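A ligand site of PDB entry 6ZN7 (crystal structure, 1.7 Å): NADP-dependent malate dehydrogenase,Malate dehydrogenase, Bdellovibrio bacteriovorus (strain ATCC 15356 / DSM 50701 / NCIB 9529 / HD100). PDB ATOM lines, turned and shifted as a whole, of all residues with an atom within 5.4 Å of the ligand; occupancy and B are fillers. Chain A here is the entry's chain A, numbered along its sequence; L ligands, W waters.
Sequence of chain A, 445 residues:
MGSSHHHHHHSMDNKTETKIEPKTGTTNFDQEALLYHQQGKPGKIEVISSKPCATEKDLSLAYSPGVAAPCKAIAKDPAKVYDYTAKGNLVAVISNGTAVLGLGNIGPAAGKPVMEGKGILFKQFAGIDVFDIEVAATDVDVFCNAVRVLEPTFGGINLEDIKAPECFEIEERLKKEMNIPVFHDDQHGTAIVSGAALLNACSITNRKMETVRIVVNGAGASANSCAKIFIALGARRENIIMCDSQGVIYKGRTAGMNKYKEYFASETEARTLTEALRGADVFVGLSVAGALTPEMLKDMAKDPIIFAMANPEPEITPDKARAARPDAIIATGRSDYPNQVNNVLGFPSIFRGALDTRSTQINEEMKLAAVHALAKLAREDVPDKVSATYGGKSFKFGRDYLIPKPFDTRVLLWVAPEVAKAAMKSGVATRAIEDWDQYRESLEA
Water W4 bridges an oxygen (O1) of the ligand (2.6 Å) and the backbone NH of Ala 164 (3.1 Å).
Water W5 lies within hydrogen-bond range of a nitrogen (N4) of the ligand and the side-chain amide nitrogen of Asn 217.
Water W9 lies within hydrogen-bond range of O9 of the ligand (2.8 Å), N of Gly 220 (2.8 Å), O of Leu 286 (3.0 Å) and N of Ala 223 (3.5 Å).
The backbone NH (N) of Ser 245 sits at hydrogen-bond distance from an oxygen (O6) of the ligand.
The side-chain hydroxyl (OG) of Ser 245 is in hydrogen-bond range of an oxygen (O16) of the ligand (2.5 Å).
The backbone NH of Ala 219 is in hydrogen-bond range of an oxygen (O5) of the ligand (2.8 Å).
O of Val 341 is in hydrogen-bond range of N7 of the ligand (2.8 Å).
A nitrogen (N7) of the ligand lies close to the side-chain hydroxyl (OG1) of Thr 190 (2.9 Å).
NZ of Lys 261 lies within salt-bridge range of O17 of the ligand (2.9 Å).
O12 of the ligand lies within hydrogen-bond range of N of Asn 311 (3.2 Å).
The side-chain amide nitrogen (ND2) of Asn 311 sits close to an oxygen (O14) of the ligand, at 3.2 Å.
An oxygen (O5) of the ligand is in hydrogen-bond range of the backbone NH (N) of Gly 220, at 3.2 Å.
The backbone NH (N) of Ser 222 is in hydrogen-bond range of an oxygen (O9) of the ligand, 3.4 Å away.
The side-chain hydroxyl (OG) of Ser 222 is in hydrogen-bond range of an oxygen (O9) of the ligand, at 3.2 Å.
O1 of the ligand is in hydrogen-bond range of N of Ala 221 (3.2 Å).
The side-chain amide oxygen of Asn 343 is in hydrogen-bond range of a nitrogen (N7) of the ligand (3.3 Å).
The backbone carbonyl oxygen (O) of Ser 287 sits at hydrogen-bond distance from an oxygen (O12) of the ligand, 3.3 Å away.
Residues that only touch the ligand: Asn 217 (3.4 Å), Gly 218 (3.9 Å), Asp 244 (3.5 Å), Leu 286 (3.4 Å), Val 288 (3.5 Å), Met 309 (3.0 Å), Ala 310 (3.5 Å) and Gly 333 (3.3 Å).
Hydrophobic or aromatic side chains within 4 Å of the ligand: Ala 219, Ala 221, Leu 286, Val 288, Ala 310 and Val 341.
Within 4 Å of the ligand: Thr 190, Asn 217, Gly 218, Ala 219, Gly 220, Ala 221, Ser 222, Asp 244, Ser 245, Lys 261, Leu 286, Ser 287, Val 288, Met 309, Ala 310, Asn 311, Gly 333, Val 341 and Asn 343.
The side-chain hydroxyl (OG1) of Thr 190 lies within hydrogen-bond range of the side-chain amide oxygen (OD1) of Asn 343 (3.2 Å).
NZ of Lys 261 is in salt-bridge range of OD2 of Asp 244, 3.1 Å away.
O of Met 309 sits at hydrogen-bond distance from ND2 of Asn 311 (3.1 Å).
N of Met 309 lies within hydrogen-bond range of O of Gly 285 (2.9 Å).
The side-chain hydroxyl (OG) of Ser 287 lies within hydrogen-bond range of the side-chain amide nitrogen (ND2) of Asn 217 (3.0 Å).
The backbone carbonyl oxygen (O) of Asn 217 is in hydrogen-bond range of the backbone NH (N) of Leu 286 (2.8 Å).
The backbone NH (N) of Ala 310 lies within hydrogen-bond range of the backbone carbonyl oxygen (O) of Gly 285 (3.5 Å).
The backbone carbonyl oxygen (O) of Cys 243 sits at hydrogen-bond distance from the backbone NH (N) of Gly 218 (2.6 Å).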
ATOM      1  N   ALA A 164     -19.171   9.718   5.721  1.00  0.00           N
ATOM      2  CA  ALA A 164     -19.412   9.759   4.281  1.00  0.00           C
ATOM      3  C   ALA A 164     -18.122  10.176   3.564  1.00  0.00           C
ATOM      4  O   ALA A 164     -17.328  10.946   4.111  1.00  0.00           O
ATOM      5  CB  ALA A 164     -20.537  10.734   3.954  1.00  0.00           C
ATOM      6  N   ASP A 186     -27.693   7.005  10.607  1.00  0.00           N
ATOM      7  CA  ASP A 186     -27.309   8.381  10.278  1.00  0.00           C
ATOM      8  C   ASP A 186     -27.824   8.782   8.902  1.00  0.00           C
ATOM      9  O   ASP A 186     -28.184   9.942   8.679  1.00  0.00           O
ATOM     10  CB  ASP A 186     -25.804   8.546  10.320  1.00  0.00           C
ATOM     11  CG  ASP A 186     -25.245   8.373  11.714  1.00  0.00           C
ATOM     12  OD1 ASP A 186     -24.980   9.389  12.380  1.00  0.00           O
ATOM     13  OD2 ASP A 186     -25.085   7.214  12.116  1.00  0.00           O
ATOM     14  N   THR A 190     -32.881  10.223   9.851  1.00  0.00           N
ATOM     15  CA  THR A 190     -33.270  11.606   9.714  1.00  0.00           C
ATOM     16  C   THR A 190     -34.164  11.802   8.495  1.00  0.00           C
ATOM     17  O   THR A 190     -35.113  12.584   8.547  1.00  0.00           O
ATOM     18  CB  THR A 190     -32.049  12.523   9.599  1.00  0.00           C
ATOM     19  OG1 THR A 190     -31.940  13.299  10.793  1.00  0.00           O
ATOM     20  CG2 THR A 190     -32.205  13.472   8.431  1.00  0.00           C
ATOM     21  N   ASN A 217     -29.439  21.997   2.353  1.00  0.00           N
ATOM     22  CA  ASN A 217     -28.131  22.580   2.625  1.00  0.00           C
ATOM     23  C   ASN A 217     -27.252  21.546   3.314  1.00  0.00           C
ATOM     24  O   ASN A 217     -27.503  21.179   4.464  1.00  0.00           O
ATOM     25  CB  ASN A 217     -28.249  23.841   3.481  1.00  0.00           C
ATOM     26  CG  ASN A 217     -27.007  24.714   3.395  1.00  0.00           C
ATOM     27  OD1 ASN A 217     -26.430  24.889   2.324  1.00  0.00           O
ATOM     28  ND2 ASN A 217     -26.569  25.254   4.534  1.00  0.00           N
ATOM     29  N   GLY A 218     -26.239  21.077   2.601  1.00  0.00           N
ATOM     30  CA  GLY A 218     -25.433  19.969   3.087  1.00  0.00           C
ATOM     31  C   GLY A 218     -25.602  18.780   2.144  1.00  0.00           C
ATOM     32  O   GLY A 218     -26.650  18.623   1.530  1.00  0.00           O
ATOM     33  N   ALA A 219     -24.559  17.967   2.030  1.00  0.00           N
ATOM     34  CA  ALA A 219     -24.604  16.845   1.104  1.00  0.00           C
ATOM     35  C   ALA A 219     -23.879  15.647   1.698  1.00  0.00           C
ATOM     36  O   ALA A 219     -23.282  14.843   0.980  1.00  0.00           O
ATOM     37  CB  ALA A 219     -23.975  17.241  -0.236  1.00  0.00           C
ATOM     38  N   GLY A 220     -23.953  15.535   3.024  1.00  0.00           N
ATOM     39  CA  GLY A 220     -23.309  14.445   3.734  1.00  0.00           C
ATOM     40  C   GLY A 220     -24.175  13.219   3.891  1.00  0.00           C
ATOM     41  O   GLY A 220     -25.078  12.963   3.073  1.00  0.00           O
ATOM     42  N   ALA A 221     -23.913  12.469   4.954  1.00  0.00           N
ATOM     43  CA  ALA A 221     -24.584  11.195   5.200  1.00  0.00           C
ATOM     44  C   ALA A 221     -26.094  11.319   5.248  1.00  0.00           C
ATOM     45  O   ALA A 221     -26.824  10.529   4.618  1.00  0.00           O
ATOM     46  CB  ALA A 221     -24.052  10.590   6.508  1.00  0.00           C
ATOM     47  N   SER A 222     -26.572  12.295   5.969  1.00  0.00           N
ATOM     48  CA  SER A 222     -27.990  12.399   6.127  1.00  0.00           C
ATOM     49  C   SER A 222     -28.701  13.130   5.041  1.00  0.00           C
ATOM     50  O   SER A 222     -29.812  12.880   4.782  1.00  0.00           O
ATOM     51  CB  SER A 222     -28.310  13.002   7.455  1.00  0.00           C
ATOM     52  OG  SER A 222     -27.788  14.277   7.519  1.00  0.00           O
ATOM     53  N   ALA A 223     -28.010  14.076   4.436  1.00  0.00           N
ATOM     54  CA  ALA A 223     -28.627  14.895   3.426  1.00  0.00           C
ATOM     55  C   ALA A 223     -29.035  14.148   2.207  1.00  0.00           C
ATOM     56  O   ALA A 223     -30.060  14.345   1.655  1.00  0.00           O
ATOM     57  CB  ALA A 223     -27.699  16.026   3.079  1.00  0.00           C
ATOM     58  N   CYS A 243     -27.098  22.004  -1.827  1.00  0.00           N
ATOM     59  CA  CYS A 243     -25.911  22.844  -1.676  1.00  0.00           C
ATOM     60  C   CYS A 243     -24.923  22.208  -0.725  1.00  0.00           C
ATOM     61  O   CYS A 243     -25.312  21.445   0.165  1.00  0.00           O
ATOM     62  CB  CYS A 243     -26.297  24.230  -1.156  1.00  0.00           C
ATOM     63  SG  CYS A 243     -27.474  25.093  -2.174  1.00  0.00           S
ATOM     64  N   ASP A 244     -23.641  22.518  -0.894  1.00  0.00           N
ATOM     65  CA  ASP A 244     -22.634  22.051   0.038  1.00  0.00           C
ATOM     66  C   ASP A 244     -21.711  23.201   0.417  1.00  0.00           C
ATOM     67  O   ASP A 244     -22.073  24.370   0.265  1.00  0.00           O
ATOM     68  CB  ASP A 244     -21.827  20.870  -0.540  1.00  0.00           C
ATOM     69  CG  ASP A 244     -21.096  21.219  -1.826  1.00  0.00           C
ATOM     70  OD1 ASP A 244     -21.047  22.402  -2.198  1.00  0.00           O
ATOM     71  OD2 ASP A 244     -20.569  20.288  -2.469  1.00  0.00           O
ATOM     72  N   SER A 245     -20.518  22.863   0.905  1.00  0.00           N
ATOM     73  CA  SER A 245     -19.585  23.872   1.398  1.00  0.00           C
ATOM     74  C   SER A 245     -19.119  24.821   0.306  1.00  0.00           C
ATOM     75  O   SER A 245     -18.554  25.876   0.590  1.00  0.00           O
ATOM     76  CB  SER A 245     -18.377  23.211   2.060  1.00  0.00           C
ATOM     77  OG  SER A 245     -17.616  22.449   1.124  1.00  0.00           O
ATOM     78  N   GLN A 246     -19.353  24.460  -0.952  1.00  0.00           N
ATOM     79  CA  GLN A 246     -18.941  25.312  -2.059  1.00  0.00           C
ATOM     80  C   GLN A 246     -20.130  25.896  -2.808  1.00  0.00           C
ATOM     81  O   GLN A 246     -19.977  26.425  -3.916  1.00  0.00           O
ATOM     82  CB  GLN A 246     -18.056  24.528  -3.020  1.00  0.00           C
ATOM     83  CG  GLN A 246     -16.708  24.173  -2.438  1.00  0.00           C
ATOM     84  CD  GLN A 246     -15.771  23.608  -3.483  1.00  0.00           C
ATOM     85  OE1 GLN A 246     -15.237  24.339  -4.315  1.00  0.00           O
ATOM     86  NE2 GLN A 246     -15.571  22.293  -3.449  1.00  0.00           N
ATOM     87  N   LYS A 261     -23.091  13.184  -4.963  1.00  0.00           N
ATOM     88  CA  LYS A 261     -23.469  14.558  -5.232  1.00  0.00           C
ATOM     89  C   LYS A 261     -23.934  14.703  -6.678  1.00  0.00           C
ATOM     90  O   LYS A 261     -24.879  15.439  -6.956  1.00  0.00           O
ATOM     91  CB  LYS A 261     -22.299  15.510  -4.971  1.00  0.00           C
ATOM     92  CG  LYS A 261     -21.856  15.554  -3.525  1.00  0.00           C
ATOM     93  CD  LYS A 261     -20.813  16.626  -3.322  1.00  0.00           C
ATOM     94  CE  LYS A 261     -20.418  16.711  -1.861  1.00  0.00           C
ATOM     95  NZ  LYS A 261     -19.254  17.620  -1.662  1.00  0.00           N
ATOM     96  N   GLY A 285     -31.805  21.811   6.443  1.00  0.00           N
ATOM     97  CA  GLY A 285     -30.478  22.200   6.890  1.00  0.00           C
ATOM     98  C   GLY A 285     -29.759  21.050   7.566  1.00  0.00           C
ATOM     99  O   GLY A 285     -30.083  20.680   8.692  1.00  0.00           O
ATOM    100  N   LEU A 286     -28.792  20.482   6.859  1.00  0.00           N
ATOM    101  CA  LEU A 286     -27.976  19.390   7.381  1.00  0.00           C
ATOM    102  C   LEU A 286     -26.517  19.755   7.186  1.00  0.00           C
ATOM    103  O   LEU A 286     -25.764  19.040   6.518  1.00  0.00           O
ATOM    104  CB  LEU A 286     -28.311  18.087   6.661  1.00  0.00           C
ATOM    105  CG  LEU A 286     -29.702  17.516   6.917  1.00  0.00           C
ATOM    106  CD1 LEU A 286     -30.036  16.485   5.859  1.00  0.00           C
ATOM    107  CD2 LEU A 286     -29.788  16.897   8.307  1.00  0.00           C
ATOM    108  N   SER A 287     -26.135  20.885   7.755  1.00  0.00           N
ATOM    109  CA  SER A 287     -24.828  21.472   7.502  1.00  0.00           C
ATOM    110  C   SER A 287     -24.204  21.978   8.789  1.00  0.00           C
ATOM    111  O   SER A 287     -23.712  21.204   9.604  1.00  0.00           O
ATOM    112  CB  SER A 287     -24.947  22.605   6.475  1.00  0.00           C
ATOM    113  OG  SER A 287     -25.870  23.608   6.896  1.00  0.00           O
ATOM    114  N   VAL A 288     -24.239  23.290   8.980  1.00  0.00           N
ATOM    115  CA  VAL A 288     -23.592  23.922  10.124  1.00  0.00           C
ATOM    116  C   VAL A 288     -24.378  25.148  10.577  1.00  0.00           C
ATOM    117  O   VAL A 288     -25.200  25.682   9.832  1.00  0.00           O
ATOM    118  CB  VAL A 288     -22.156  24.329   9.788  1.00  0.00           C
ATOM    119  CG1 VAL A 288     -21.298  23.092   9.548  1.00  0.00           C
ATOM    120  CG2 VAL A 288     -22.139  25.243   8.574  1.00  0.00           C
ATOM    121  N   ALA A 291     -25.772  28.986   9.009  1.00  0.00           N
ATOM    122  CA  ALA A 291     -25.720  28.889   7.557  1.00  0.00           C
ATOM    123  C   ALA A 291     -26.922  29.543   6.896  1.00  0.00           C
ATOM    124  O   ALA A 291     -26.863  29.944   5.722  1.00  0.00           O
ATOM    125  CB  ALA A 291     -25.628  27.427   7.129  1.00  0.00           C
ATOM    126  N   MET A 309     -31.481  21.551  11.122  1.00  0.00           N
ATOM    127  CA  MET A 309     -31.163  20.400  11.953  1.00  0.00           C
ATOM    128  C   MET A 309     -29.675  20.285  12.295  1.00  0.00           C
ATOM    129  O   MET A 309     -29.273  19.311  12.925  1.00  0.00           O
ATOM    130  CB  MET A 309     -31.670  19.121  11.293  1.00  0.00           C
ATOM    131  CG  MET A 309     -33.191  19.055  11.270  1.00  0.00           C
ATOM    132  SD  MET A 309     -33.825  17.710  10.245  1.00  0.00           S
ATOM    133  CE  MET A 309     -33.227  18.190   8.631  1.00  0.00           C
ATOM    134  N   ALA A 310     -28.881  21.280  11.918  1.00  0.00           N
ATOM    135  CA  ALA A 310     -27.482  21.314  12.337  1.00  0.00           C
ATOM    136  C   ALA A 310     -27.400  21.258  13.854  1.00  0.00           C
ATOM    137  O   ALA A 310     -28.180  21.909  14.559  1.00  0.00           O
ATOM    138  CB  ALA A 310     -26.797  22.574  11.805  1.00  0.00           C
ATOM    139  N   ASN A 311     -26.475  20.467  14.372  1.00  0.00           N
ATOM    140  CA  ASN A 311     -26.251  20.367  15.806  1.00  0.00           C
ATOM    141  C   ASN A 311     -24.809  20.728  16.168  1.00  0.00           C
ATOM    142  O   ASN A 311     -23.901  20.470  15.385  1.00  0.00           O
ATOM    143  CB  ASN A 311     -26.588  18.964  16.312  1.00  0.00           C
ATOM    144  CG  ASN A 311     -28.053  18.607  16.125  1.00  0.00           C
ATOM    145  OD1 ASN A 311     -28.935  19.263  16.682  1.00  0.00           O
ATOM    146  ND2 ASN A 311     -28.311  17.566  15.351  1.00  0.00           N
ATOM    147  N   THR A 332     -36.245  21.601  14.181  1.00  0.00           N
ATOM    148  CA  THR A 332     -34.806  21.532  14.405  1.00  0.00           C
ATOM    149  C   THR A 332     -34.428  20.176  14.978  1.00  0.00           C
ATOM    150  O   THR A 332     -35.295  19.318  15.156  1.00  0.00           O
ATOM    151  CB  THR A 332     -34.305  22.639  15.361  1.00  0.00           C
ATOM    152  OG1 THR A 332     -34.536  22.254  16.719  1.00  0.00           O
ATOM    153  CG2 THR A 332     -35.020  23.949  15.070  1.00  0.00           C
ATOM    154  N   GLY A 333     -33.151  19.989  15.272  1.00  0.00           N
ATOM    155  CA  GLY A 333     -32.676  18.758  15.861  1.00  0.00           C
ATOM    156  C   GLY A 333     -32.668  18.798  17.383  1.00  0.00           C
ATOM    157  O   GLY A 333     -32.271  17.835  18.032  1.00  0.00           O
ATOM    158  N   VAL A 341     -36.828  16.916  15.157  1.00  0.00           N
ATOM    159  CA  VAL A 341     -36.536  15.805  14.274  1.00  0.00           C
ATOM    160  C   VAL A 341     -35.532  14.895  14.977  1.00  0.00           C
ATOM    161  O   VAL A 341     -34.324  15.051  14.828  1.00  0.00           O
ATOM    162  CB  VAL A 341     -35.991  16.273  12.924  1.00  0.00           C
ATOM    163  CG1 VAL A 341     -35.594  15.085  12.061  1.00  0.00           C
ATOM    164  CG2 VAL A 341     -37.032  17.147  12.222  1.00  0.00           C
ATOM    165  N   ASN A 342     -36.054  13.958  15.763  1.00  0.00           N
ATOM    166  CA  ASN A 342     -35.251  13.086  16.616  1.00  0.00           C
ATOM    167  C   ASN A 342     -35.215  11.664  16.070  1.00  0.00           C
ATOM    168  O   ASN A 342     -36.267  11.041  15.931  1.00  0.00           O
ATOM    169  CB  ASN A 342     -35.809  13.122  18.049  1.00  0.00           C
ATOM    170  CG  ASN A 342     -34.925  12.423  19.063  1.00  0.00           C
ATOM    171  OD1 ASN A 342     -34.319  11.399  18.784  1.00  0.00           O
ATOM    172  ND2 ASN A 342     -34.872  12.992  20.267  1.00  0.00           N
ATOM    173  N   ASN A 343     -34.018  11.144  15.786  1.00  0.00           N
ATOM    174  CA  ASN A 343     -33.873   9.840  15.133  1.00  0.00           C
ATOM    175  C   ASN A 343     -34.463   8.703  15.958  1.00  0.00           C
ATOM    176  O   ASN A 343     -34.756   7.623  15.422  1.00  0.00           O
ATOM    177  CB  ASN A 343     -32.394   9.520  14.824  1.00  0.00           C
ATOM    178  CG  ASN A 343     -31.927  10.128  13.510  1.00  0.00           C
ATOM    179  OD1 ASN A 343     -32.342  11.226  13.141  1.00  0.00           O
ATOM    180  ND2 ASN A 343     -31.065   9.412  12.782  1.00  0.00           N
HETATM  181  P1  LIG L   1     -21.592  15.104   7.194  1.00  0.00           P
HETATM  182  O1  LIG L   1     -21.614  13.736   6.723  1.00  0.00           O
HETATM  183  O2  LIG L   1     -20.279  15.494   7.643  1.00  0.00           O
HETATM  184  O3  LIG L   1     -21.939  16.066   6.038  1.00  0.00           O
HETATM  185  C1  LIG L   1     -21.489  17.418   6.152  1.00  0.00           C
HETATM  186  C2  LIG L   1     -22.095  18.215   5.012  1.00  0.00           C
HETATM  187  O4  LIG L   1     -22.149  19.465   5.372  1.00  0.00           O
HETATM  188  C3  LIG L   1     -21.181  18.153   3.815  1.00  0.00           C
HETATM  189  O5  LIG L   1     -21.853  17.951   2.709  1.00  0.00           O
HETATM  190  C4  LIG L   1     -20.495  19.551   3.828  1.00  0.00           C
HETATM  191  O6  LIG L   1     -20.056  19.921   2.518  1.00  0.00           O
HETATM  192  C5  LIG L   1     -21.472  20.313   4.204  1.00  0.00           C
HETATM  193  N1  LIG L   1     -21.032  21.577   4.729  1.00  0.00           N
HETATM  194  C6  LIG L   1     -20.000  21.942   5.523  1.00  0.00           C
HETATM  195  N2  LIG L   1     -20.077  23.283   5.711  1.00  0.00           N
HETATM  196  C7  LIG L   1     -21.152  23.748   5.021  1.00  0.00           C
HETATM  197  C8  LIG L   1     -21.680  25.011   4.891  1.00  0.00           C
HETATM  198  N3  LIG L   1     -21.327  26.296   5.376  1.00  0.00           N
HETATM  199  N4  LIG L   1     -22.783  25.199   4.132  1.00  0.00           N
HETATM  200  C9  LIG L   1     -23.364  24.138   3.531  1.00  0.00           C
HETATM  201  N5  LIG L   1     -22.828  22.883   3.669  1.00  0.00           N
HETATM  202  C10 LIG L   1     -21.740  22.707   4.416  1.00  0.00           C
HETATM  203  O7  LIG L   1     -22.505  15.314   8.441  1.00  0.00           O
HETATM  204  P2  LIG L   1     -23.875  14.752   8.703  1.00  0.00           P
HETATM  205  O8  LIG L   1     -23.791  13.504   9.379  1.00  0.00           O
HETATM  206  O9  LIG L   1     -24.658  14.674   7.466  1.00  0.00           O
HETATM  207  O10 LIG L   1     -24.513  15.787   9.640  1.00  0.00           O
HETATM  208  C11 LIG L   1     -24.596  17.076   9.048  1.00  0.00           C
HETATM  209  C12 LIG L   1     -25.304  18.090  10.016  1.00  0.00           C
HETATM  210  O11 LIG L   1     -26.541  17.734  10.140  1.00  0.00           O
HETATM  211  C13 LIG L   1     -24.681  17.973  11.372  1.00  0.00           C
HETATM  212  O12 LIG L   1     -24.737  19.156  12.045  1.00  0.00           O
HETATM  213  C14 LIG L   1     -25.603  16.982  12.046  1.00  0.00           C
HETATM  214  O13 LIG L   1     -25.397  17.084  13.539  1.00  0.00           O
HETATM  215  C15 LIG L   1     -26.768  17.332  11.646  1.00  0.00           C
HETATM  216  N6  LIG L   1     -27.698  16.274  11.740  1.00  0.00           N
HETATM  217  C16 LIG L   1     -28.817  16.397  12.518  1.00  0.00           C
HETATM  218  C17 LIG L   1     -29.728  15.364  12.656  1.00  0.00           C
HETATM  219  C18 LIG L   1     -30.963  15.442  13.515  1.00  0.00           C
HETATM  220  O14 LIG L   1     -31.108  16.313  14.276  1.00  0.00           O
HETATM  221  N7  LIG L   1     -31.930  14.437  13.456  1.00  0.00           N
HETATM  222  C19 LIG L   1     -29.500  14.196  11.997  1.00  0.00           C
HETATM  223  C20 LIG L   1     -28.402  14.055  11.234  1.00  0.00           C
HETATM  224  C21 LIG L   1     -27.505  15.102  11.094  1.00  0.00           C
HETATM  225  P3  LIG L   1     -18.885  19.261   1.836  1.00  0.00           P
HETATM  226  O15 LIG L   1     -17.850  19.004   2.863  1.00  0.00           O
HETATM  227  O16 LIG L   1     -18.408  20.135   0.832  1.00  0.00           O
HETATM  228  O17 LIG L   1     -19.246  18.029   1.206  1.00  0.00           O
HETATM  229  O   HOH W   1     -27.985  11.066  12.635  1.00  0.00           O
HETATM  230  O   HOH W   2     -22.156  28.854   5.080  1.00  0.00           O
HETATM  231  O   HOH W   3     -21.780  11.664   9.699  1.00  0.00           O
HETATM  232  O   HOH W   4     -19.743  12.144   7.553  1.00  0.00           O
HETATM  233  O   HOH W   5     -24.510  27.191   3.447  1.00  0.00           O
HETATM  234  O   HOH W   6     -31.517  15.395  16.888  1.00  0.00           O
HETATM  235  O   HOH W   7     -19.736  14.721   2.152  1.00  0.00           O
HETATM  236  O   HOH W   8     -25.724  11.719  11.594  1.00  0.00           O
HETATM  237  O   HOH W   9     -25.458  16.281   5.306  1.00  0.00           O
